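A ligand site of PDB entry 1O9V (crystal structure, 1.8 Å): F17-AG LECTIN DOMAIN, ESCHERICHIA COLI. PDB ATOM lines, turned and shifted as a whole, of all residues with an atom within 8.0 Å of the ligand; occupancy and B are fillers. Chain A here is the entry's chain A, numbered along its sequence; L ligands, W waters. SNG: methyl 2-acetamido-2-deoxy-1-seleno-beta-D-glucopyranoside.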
ATOM      1  N   GLN A  41     -29.017 -16.496   6.593  1.00  0.00           N
ATOM      2  CA  GLN A  41     -29.114 -17.651   7.458  1.00  0.00           C
ATOM      3  C   GLN A  41     -30.139 -18.610   6.852  1.00  0.00           C
ATOM      4  O   GLN A  41     -31.218 -18.190   6.397  1.00  0.00           O
ATOM      5  CB  GLN A  41     -29.624 -17.204   8.840  1.00  0.00           C
ATOM      6  CG  GLN A  41     -29.864 -18.340   9.805  1.00  0.00           C
ATOM      7  CD  GLN A  41     -30.450 -17.855  11.120  1.00  0.00           C
ATOM      8  OE1 GLN A  41     -31.578 -17.328  11.178  1.00  0.00           O
ATOM      9  NE2 GLN A  41     -29.672 -17.987  12.181  1.00  0.00           N
ATOM     10  N   ASN A  42     -29.816 -19.888   6.864  1.00  0.00           N
ATOM     11  CA  ASN A  42     -30.774 -20.890   6.373  1.00  0.00           C
ATOM     12  C   ASN A  42     -30.483 -22.178   7.128  1.00  0.00           C
ATOM     13  O   ASN A  42     -29.392 -22.717   7.010  1.00  0.00           O
ATOM     14  CB  ASN A  42     -30.597 -21.124   4.890  1.00  0.00           C
ATOM     15  CG  ASN A  42     -31.709 -21.988   4.290  1.00  0.00           C
ATOM     16  OD1 ASN A  42     -32.422 -22.734   4.997  1.00  0.00           O
ATOM     17  ND2 ASN A  42     -31.847 -21.905   2.981  1.00  0.00           N
ATOM     18  N   ALA A  43     -31.432 -22.651   7.941  1.00  0.00           N
ATOM     19  CA  ALA A  43     -31.230 -23.866   8.722  1.00  0.00           C
ATOM     20  C   ALA A  43     -31.259 -25.129   7.869  1.00  0.00           C
ATOM     21  O   ALA A  43     -30.808 -26.170   8.333  1.00  0.00           O
ATOM     22  CB  ALA A  43     -32.353 -23.994   9.797  1.00  0.00           C
ATOM     23  N   ASN A  44     -31.760 -24.998   6.633  1.00  0.00           N
ATOM     24  CA  ASN A  44     -31.987 -26.151   5.781  1.00  0.00           C
ATOM     25  C   ASN A  44     -31.340 -26.102   4.418  1.00  0.00           C
ATOM     26  O   ASN A  44     -31.958 -25.733   3.399  1.00  0.00           O
ATOM     27  CB  ASN A  44     -33.501 -26.312   5.654  1.00  0.00           C
ATOM     28  CG  ASN A  44     -34.233 -26.008   6.965  1.00  0.00           C
ATOM     29  OD1 ASN A  44     -34.985 -25.006   7.063  1.00  0.00           O
ATOM     30  ND2 ASN A  44     -34.003 -26.825   7.974  1.00  0.00           N
ATOM     31  N   VAL A  45     -30.065 -26.460   4.392  1.00  0.00           N
ATOM     32  CA  VAL A  45     -29.349 -26.442   3.152  1.00  0.00           C
ATOM     33  C   VAL A  45     -29.115 -27.876   2.697  1.00  0.00           C
ATOM     34  O   VAL A  45     -29.117 -28.151   1.491  1.00  0.00           O
ATOM     35  CB  VAL A  45     -28.038 -25.644   3.342  1.00  0.00           C
ATOM     36  CG1 VAL A  45     -27.231 -25.612   2.023  1.00  0.00           C
ATOM     37  CG2 VAL A  45     -28.410 -24.206   3.803  1.00  0.00           C
ATOM     38  N   TRP A  46     -28.920 -28.790   3.641  1.00  0.00           N
ATOM     39  CA  TRP A  46     -28.790 -30.191   3.302  1.00  0.00           C
ATOM     40  C   TRP A  46     -29.691 -30.968   4.238  1.00  0.00           C
ATOM     41  O   TRP A  46     -29.873 -30.610   5.401  1.00  0.00           O
ATOM     42  CB  TRP A  46     -27.344 -30.717   3.512  1.00  0.00           C
ATOM     43  CG  TRP A  46     -26.353 -30.203   2.534  1.00  0.00           C
ATOM     44  CD1 TRP A  46     -26.111 -30.686   1.275  1.00  0.00           C
ATOM     45  CD2 TRP A  46     -25.549 -29.055   2.689  1.00  0.00           C
ATOM     46  NE1 TRP A  46     -25.198 -29.880   0.640  1.00  0.00           N
ATOM     47  CE2 TRP A  46     -24.846 -28.863   1.493  1.00  0.00           C
ATOM     48  CE3 TRP A  46     -25.353 -28.131   3.747  1.00  0.00           C
ATOM     49  CZ2 TRP A  46     -23.952 -27.811   1.308  1.00  0.00           C
ATOM     50  CZ3 TRP A  46     -24.485 -27.110   3.553  1.00  0.00           C
ATOM     51  CH2 TRP A  46     -23.791 -26.953   2.347  1.00  0.00           C
ATOM     52  N   ILE A  48     -30.018 -34.554   6.102  1.00  0.00           N
ATOM     53  CA  ILE A  48     -29.113 -35.641   6.457  1.00  0.00           C
ATOM     54  C   ILE A  48     -29.847 -36.665   7.347  1.00  0.00           C
ATOM     55  O   ILE A  48     -30.777 -36.309   8.068  1.00  0.00           O
ATOM     56  CB  ILE A  48     -27.870 -35.085   7.176  1.00  0.00           C
ATOM     57  CG1 ILE A  48     -28.252 -34.485   8.531  1.00  0.00           C
ATOM     58  CG2 ILE A  48     -27.125 -34.002   6.261  1.00  0.00           C
ATOM     59  CD1 ILE A  48     -26.999 -33.960   9.370  1.00  0.00           C
ATOM     60  N   VAL A  54     -21.480 -34.388   9.646  1.00  0.00           N
ATOM     61  CA  VAL A  54     -21.085 -33.284   8.774  1.00  0.00           C
ATOM     62  C   VAL A  54     -20.825 -31.954   9.445  1.00  0.00           C
ATOM     63  O   VAL A  54     -21.495 -31.596  10.402  1.00  0.00           O
ATOM     64  CB  VAL A  54     -22.168 -33.069   7.663  1.00  0.00           C
ATOM     65  CG1 VAL A  54     -23.455 -32.487   8.246  1.00  0.00           C
ATOM     66  CG2 VAL A  54     -21.674 -32.137   6.598  1.00  0.00           C
ATOM     67  N   LEU A  56     -18.781 -27.802   8.372  1.00  0.00           N
ATOM     68  CA  LEU A  56     -18.717 -26.801   7.284  1.00  0.00           C
ATOM     69  C   LEU A  56     -17.351 -26.144   7.123  1.00  0.00           C
ATOM     70  O   LEU A  56     -16.705 -25.832   8.121  1.00  0.00           O
ATOM     71  CB  LEU A  56     -19.658 -25.607   7.564  1.00  0.00           C
ATOM     72  CG  LEU A  56     -21.130 -25.932   7.750  1.00  0.00           C
ATOM     73  CD1 LEU A  56     -21.887 -24.688   8.249  1.00  0.00           C
ATOM     74  CD2 LEU A  56     -21.730 -26.409   6.442  1.00  0.00           C
ATOM     75  N   GLY A  87     -20.470 -19.836   9.365  1.00  0.00           N
ATOM     76  CA  GLY A  87     -20.600 -20.899  10.326  1.00  0.00           C
ATOM     77  C   GLY A  87     -21.891 -21.650  10.239  1.00  0.00           C
ATOM     78  O   GLY A  87     -22.565 -21.620   9.185  1.00  0.00           O
ATOM     79  N   ASP A  88     -22.193 -22.386  11.318  1.00  0.00           N
ATOM     80  CA  ASP A  88     -23.436 -23.147  11.447  1.00  0.00           C
ATOM     81  C   ASP A  88     -24.615 -22.159  11.475  1.00  0.00           C
ATOM     82  O   ASP A  88     -24.441 -20.906  11.499  1.00  0.00           O
ATOM     83  CB  ASP A  88     -23.403 -24.022  12.724  1.00  0.00           C
ATOM     84  CG  ASP A  88     -24.519 -25.076  12.760  1.00  0.00           C
ATOM     85  OD1 ASP A  88     -25.002 -25.528  11.680  1.00  0.00           O
ATOM     86  OD2 ASP A  88     -24.876 -25.461  13.897  1.00  0.00           O
ATOM     87  N   THR A  89     -25.826 -22.703  11.453  1.00  0.00           N
ATOM     88  CA  THR A  89     -27.034 -21.861  11.373  1.00  0.00           C
ATOM     89  C   THR A  89     -27.152 -20.643  12.292  1.00  0.00           C
ATOM     90  O   THR A  89     -27.323 -19.522  11.841  1.00  0.00           O
ATOM     91  CB  THR A  89     -28.296 -22.747  11.536  1.00  0.00           C
ATOM     92  OG1 THR A  89     -28.208 -23.838  10.607  1.00  0.00           O
ATOM     93  CG2 THR A  89     -29.549 -21.969  11.273  1.00  0.00           C
ATOM     94  N   LYS A  90     -27.036 -20.872  13.593  1.00  0.00           N
ATOM     95  CA  LYS A  90     -27.160 -19.795  14.568  1.00  0.00           C
ATOM     96  C   LYS A  90     -26.039 -18.760  14.468  1.00  0.00           C
ATOM     97  O   LYS A  90     -24.858 -19.079  14.509  1.00  0.00           O
ATOM     98  CB  LYS A  90     -27.269 -20.385  15.979  1.00  0.00           C
ATOM     99  CG  LYS A  90     -28.640 -21.045  16.119  1.00  0.00           C
ATOM    100  CD  LYS A  90     -28.843 -21.730  17.434  1.00  0.00           C
ATOM    101  CE  LYS A  90     -30.144 -22.538  17.358  1.00  0.00           C
ATOM    102  NZ  LYS A  90     -30.465 -23.222  18.623  1.00  0.00           N
ATOM    103  N   ARG A  93     -22.754 -18.790  16.522  1.00  0.00           N
ATOM    104  CA  ARG A  93     -21.757 -19.817  16.297  1.00  0.00           C
ATOM    105  C   ARG A  93     -20.808 -19.484  15.150  1.00  0.00           C
ATOM    106  O   ARG A  93     -19.970 -20.309  14.776  1.00  0.00           O
ATOM    107  CB  ARG A  93     -22.428 -21.148  16.055  1.00  0.00           C
ATOM    108  CG  ARG A  93     -22.856 -21.661  17.429  1.00  0.00           C
ATOM    109  CD  ARG A  93     -23.789 -22.784  17.373  1.00  0.00           C
ATOM    110  NE  ARG A  93     -24.619 -22.767  18.565  1.00  0.00           N
ATOM    111  CZ  ARG A  93     -25.616 -23.601  18.761  1.00  0.00           C
ATOM    112  NH1 ARG A  93     -25.887 -24.513  17.855  1.00  0.00           N
ATOM    113  NH2 ARG A  93     -26.357 -23.495  19.857  1.00  0.00           N
ATOM    114  N   PHE A 106     -17.317 -24.767  11.152  1.00  0.00           N
ATOM    115  CA  PHE A 106     -18.233 -25.506  12.010  1.00  0.00           C
ATOM    116  C   PHE A 106     -17.640 -26.890  12.132  1.00  0.00           C
ATOM    117  O   PHE A 106     -17.577 -27.627  11.142  1.00  0.00           O
ATOM    118  CB  PHE A 106     -19.650 -25.565  11.418  1.00  0.00           C
ATOM    119  CG  PHE A 106     -20.607 -26.486  12.187  1.00  0.00           C
ATOM    120  CD1 PHE A 106     -20.672 -26.464  13.581  1.00  0.00           C
ATOM    121  CD2 PHE A 106     -21.497 -27.298  11.497  1.00  0.00           C
ATOM    122  CE1 PHE A 106     -21.599 -27.223  14.282  1.00  0.00           C
ATOM    123  CE2 PHE A 106     -22.439 -28.073  12.174  1.00  0.00           C
ATOM    124  CZ  PHE A 106     -22.495 -28.037  13.584  1.00  0.00           C
ATOM    125  N   GLY A 108     -18.734 -29.565  13.351  1.00  0.00           N
ATOM    126  CA  GLY A 108     -19.611 -30.635  12.918  1.00  0.00           C
ATOM    127  C   GLY A 108     -20.456 -31.395  13.921  1.00  0.00           C
ATOM    128  O   GLY A 108     -20.269 -31.276  15.123  1.00  0.00           O
ATOM    129  N   TRP A 109     -21.429 -32.135  13.386  1.00  0.00           N
ATOM    130  CA  TRP A 109     -22.260 -32.981  14.216  1.00  0.00           C
ATOM    131  C   TRP A 109     -22.684 -34.207  13.426  1.00  0.00           C
ATOM    132  O   TRP A 109     -22.504 -34.256  12.208  1.00  0.00           O
ATOM    133  CB  TRP A 109     -23.500 -32.263  14.737  1.00  0.00           C
ATOM    134  CG  TRP A 109     -24.613 -32.073  13.737  1.00  0.00           C
ATOM    135  CD1 TRP A 109     -24.573 -31.345  12.584  1.00  0.00           C
ATOM    136  CD2 TRP A 109     -25.962 -32.522  13.881  1.00  0.00           C
ATOM    137  NE1 TRP A 109     -25.824 -31.302  12.000  1.00  0.00           N
ATOM    138  CE2 TRP A 109     -26.693 -32.010  12.785  1.00  0.00           C
ATOM    139  CE3 TRP A 109     -26.621 -33.287  14.839  1.00  0.00           C
ATOM    140  CZ2 TRP A 109     -28.065 -32.247  12.627  1.00  0.00           C
ATOM    141  CZ3 TRP A 109     -27.983 -33.509  14.682  1.00  0.00           C
ATOM    142  CH2 TRP A 109     -28.686 -32.987  13.573  1.00  0.00           C
ATOM    143  N   CYS A 110     -23.197 -35.200  14.140  1.00  0.00           N
ATOM    144  CA  CYS A 110     -23.681 -36.399  13.498  1.00  0.00           C
ATOM    145  C   CYS A 110     -25.162 -36.530  13.877  1.00  0.00           C
ATOM    146  O   CYS A 110     -25.525 -36.387  15.061  1.00  0.00           O
ATOM    147  CB  CYS A 110     -22.896 -37.597  13.981  1.00  0.00           C
ATOM    148  SG  CYS A 110     -21.109 -37.560  13.693  1.00  0.00           S
ATOM    149  N   VAL A 111     -26.021 -36.803  12.911  1.00  0.00           N
ATOM    150  CA  VAL A 111     -27.445 -36.984  13.164  1.00  0.00           C
ATOM    151  C   VAL A 111     -27.565 -38.435  13.665  1.00  0.00           C
ATOM    152  O   VAL A 111     -26.685 -39.246  13.358  1.00  0.00           O
ATOM    153  CB  VAL A 111     -28.297 -36.723  11.877  1.00  0.00           C
ATOM    154  CG1 VAL A 111     -28.005 -37.757  10.779  1.00  0.00           C
ATOM    155  CG2 VAL A 111     -29.809 -36.706  12.255  1.00  0.00           C
ATOM    156  N   ALA A 116     -33.588 -38.247  11.291  1.00  0.00           N
ATOM    157  CA  ALA A 116     -33.272 -37.335  10.193  1.00  0.00           C
ATOM    158  C   ALA A 116     -33.361 -35.893  10.685  1.00  0.00           C
ATOM    159  O   ALA A 116     -34.097 -35.579  11.628  1.00  0.00           O
ATOM    160  CB  ALA A 116     -34.278 -37.582   9.077  1.00  0.00           C
ATOM    161  N   SER A 117     -32.616 -35.020  10.050  1.00  0.00           N
ATOM    162  CA  SER A 117     -32.636 -33.612  10.389  1.00  0.00           C
ATOM    163  C   SER A 117     -32.063 -32.850   9.200  1.00  0.00           C
ATOM    164  O   SER A 117     -32.070 -33.362   8.074  1.00  0.00           O
ATOM    165  CB  SER A 117     -31.837 -33.349  11.685  1.00  0.00           C
ATOM    166  OG  SER A 117     -32.026 -31.994  12.124  1.00  0.00           O
ATOM    167  N   THR A 118     -31.622 -31.621   9.380  1.00  0.00           N
ATOM    168  CA  THR A 118     -31.055 -30.864   8.289  1.00  0.00           C
ATOM    169  C   THR A 118     -29.763 -30.197   8.740  1.00  0.00           C
ATOM    170  O   THR A 118     -29.468 -30.124   9.932  1.00  0.00           O
ATOM    171  CB  THR A 118     -31.997 -29.712   7.815  1.00  0.00           C
ATOM    172  OG1 THR A 118     -32.350 -28.937   8.967  1.00  0.00           O
ATOM    173  CG2 THR A 118     -33.253 -30.243   7.152  1.00  0.00           C
ATOM    174  N   GLN A 119     -28.962 -29.742   7.776  1.00  0.00           N
ATOM    175  CA  GLN A 119     -27.725 -29.049   8.133  1.00  0.00           C
ATOM    176  C   GLN A 119     -27.886 -27.686   7.504  1.00  0.00           C
ATOM    177  O   GLN A 119     -28.263 -27.575   6.317  1.00  0.00           O
ATOM    178  CB  GLN A 119     -26.499 -29.782   7.589  1.00  0.00           C
ATOM    179  CG  GLN A 119     -25.179 -28.989   7.680  1.00  0.00           C
ATOM    180  CD  GLN A 119     -24.868 -28.598   9.129  1.00  0.00           C
ATOM    181  OE1 GLN A 119     -24.976 -29.440  10.038  1.00  0.00           O
ATOM    182  NE2 GLN A 119     -24.473 -27.334   9.351  1.00  0.00           N
ATOM    183  N   GLY A 120     -27.615 -26.642   8.296  1.00  0.00           N
ATOM    184  CA  GLY A 120     -27.746 -25.272   7.825  1.00  0.00           C
ATOM    185  C   GLY A 120     -26.441 -24.482   7.837  1.00  0.00           C
ATOM    186  O   GLY A 120     -25.352 -25.050   7.980  1.00  0.00           O
ATOM    187  N   LEU A 121     -26.558 -23.179   7.675  1.00  0.00           N
ATOM    188  CA  LEU A 121     -25.399 -22.304   7.718  1.00  0.00           C
ATOM    189  C   LEU A 121     -25.803 -20.838   7.881  1.00  0.00           C
ATOM    190  O   LEU A 121     -26.990 -20.487   7.770  1.00  0.00           O
ATOM    191  CB  LEU A 121     -24.546 -22.449   6.436  1.00  0.00           C
ATOM    192  CG  LEU A 121     -25.319 -22.297   5.127  1.00  0.00           C
ATOM    193  CD1 LEU A 121     -25.606 -20.787   4.838  1.00  0.00           C
ATOM    194  CD2 LEU A 121     -24.474 -22.948   3.961  1.00  0.00           C
ATOM    195  N   SER A 122     -24.807 -19.996   8.146  1.00  0.00           N
ATOM    196  CA  SER A 122     -25.059 -18.558   8.231  1.00  0.00           C
ATOM    197  C   SER A 122     -23.809 -17.839   7.818  1.00  0.00           C
ATOM    198  O   SER A 122     -22.688 -18.354   7.987  1.00  0.00           O
ATOM    199  CB  SER A 122     -25.441 -18.141   9.662  1.00  0.00           C
ATOM    200  OG  SER A 122     -24.388 -18.413  10.535  1.00  0.00           O
HETATM  201  C1  SNG L   1     -30.220 -28.903  13.168  1.00  0.00           C
HETATM  202  C2  SNG L   1     -30.634 -27.597  12.471  1.00  0.00           C
HETATM  203  C3  SNG L   1     -29.550 -27.187  11.458  1.00  0.00           C
HETATM  204  C4  SNG L   1     -28.160 -27.128  12.098  1.00  0.00           C
HETATM  205  C5  SNG L   1     -27.876 -28.471  12.806  1.00  0.00           C
HETATM  206  C6  SNG L   1     -26.503 -28.464  13.527  1.00  0.00           C
HETATM  207  C7  SNG L   1     -33.029 -27.141  12.003  1.00  0.00           C
HETATM  208  C8  SNG L   1     -32.957 -26.191  13.168  1.00  0.00           C
HETATM  209  CM  SNG L   1     -31.421 -27.915  15.515  1.00  0.00           C
HETATM  210  N2  SNG L   1     -31.905 -27.780  11.740  1.00  0.00           N
HETATM  211  O3  SNG L   1     -29.883 -25.888  10.907  1.00  0.00           O
HETATM  212  O4  SNG L   1     -27.190 -26.919  11.074  1.00  0.00           O
HETATM  213  O5  SNG L   1     -28.908 -28.680  13.776  1.00  0.00           O
HETATM  214  O6  SNG L   1     -26.528 -27.480  14.526  1.00  0.00           O
HETATM  215  O7  SNG L   1     -34.079 -27.234  11.303  1.00  0.00           O
HETATM  216 SE   SNG L   1     -31.455 -29.397  14.474  1.00  0.00          SE
HETATM  217  O   HOH W   1     -28.387 -30.470  16.009  1.00  0.00           O
HETATM  218  O   HOH W   2     -28.603 -25.256  15.435  1.00  0.00           O
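OG1 of Thr 118 is in hydrogen-bond range of N2 of the ligand, 3.0 Å away. O4 of the ligand is in hydrogen-bond range of OD1 of Asp 88 (2.7 Å). NE2 of Gln 119 sits at hydrogen-bond distance from O4 of the ligand, at 3.2 Å. The backbone NH (N) of Gly 120 lies within hydrogen-bond range of an oxygen (O4) of the ligand (2.8 Å). The backbone carbonyl oxygen (O) of Ala 43 sits at hydrogen-bond distance from an oxygen (O3) of the ligand. ND2 of Asn 44 lies within hydrogen-bond range of O7 of the ligand (3.4 Å). An oxygen (O3) of the ligand is in hydrogen-bond range of the side-chain hydroxyl of Thr 89 (2.7 Å).
N of Gln 119 lies within hydrogen-bond range of O of Trp 46. The backbone carbonyl oxygen of Ala 43 is in hydrogen-bond range of the side-chain hydroxyl of Thr 118 (3.2 Å). OG of Ser 122 lies within hydrogen-bond range of O of Asp 88, at 2.7 Å. The backbone carbonyl oxygen (O) of Gln 119 sits at hydrogen-bond distance from the backbone NH (N) of Val 45 (2.9 Å). N of Asn 44 lies within hydrogen-bond range of OD1 of Asn 42, 2.9 Å away. ND2 of Asn 44 is in hydrogen-bond range of OG1 of Thr 118 (2.9 Å). The backbone NH (N) of Leu 121 is in hydrogen-bond range of the side-chain hydroxyl (OG1) of Thr 89, at 3.4 Å. The side-chain amide oxygen of Gln 119 lies within hydrogen-bond range of the indole nitrogen of Trp 109 (2.8 Å).
Residues that only touch the ligand: Trp 109 and Ser 117. Within 4 Å of the ligand: Ala 43, Asn 44, Asp 88, Thr 89, Trp 109, Ser 117, Thr 118, Gln 119 and Gly 120.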
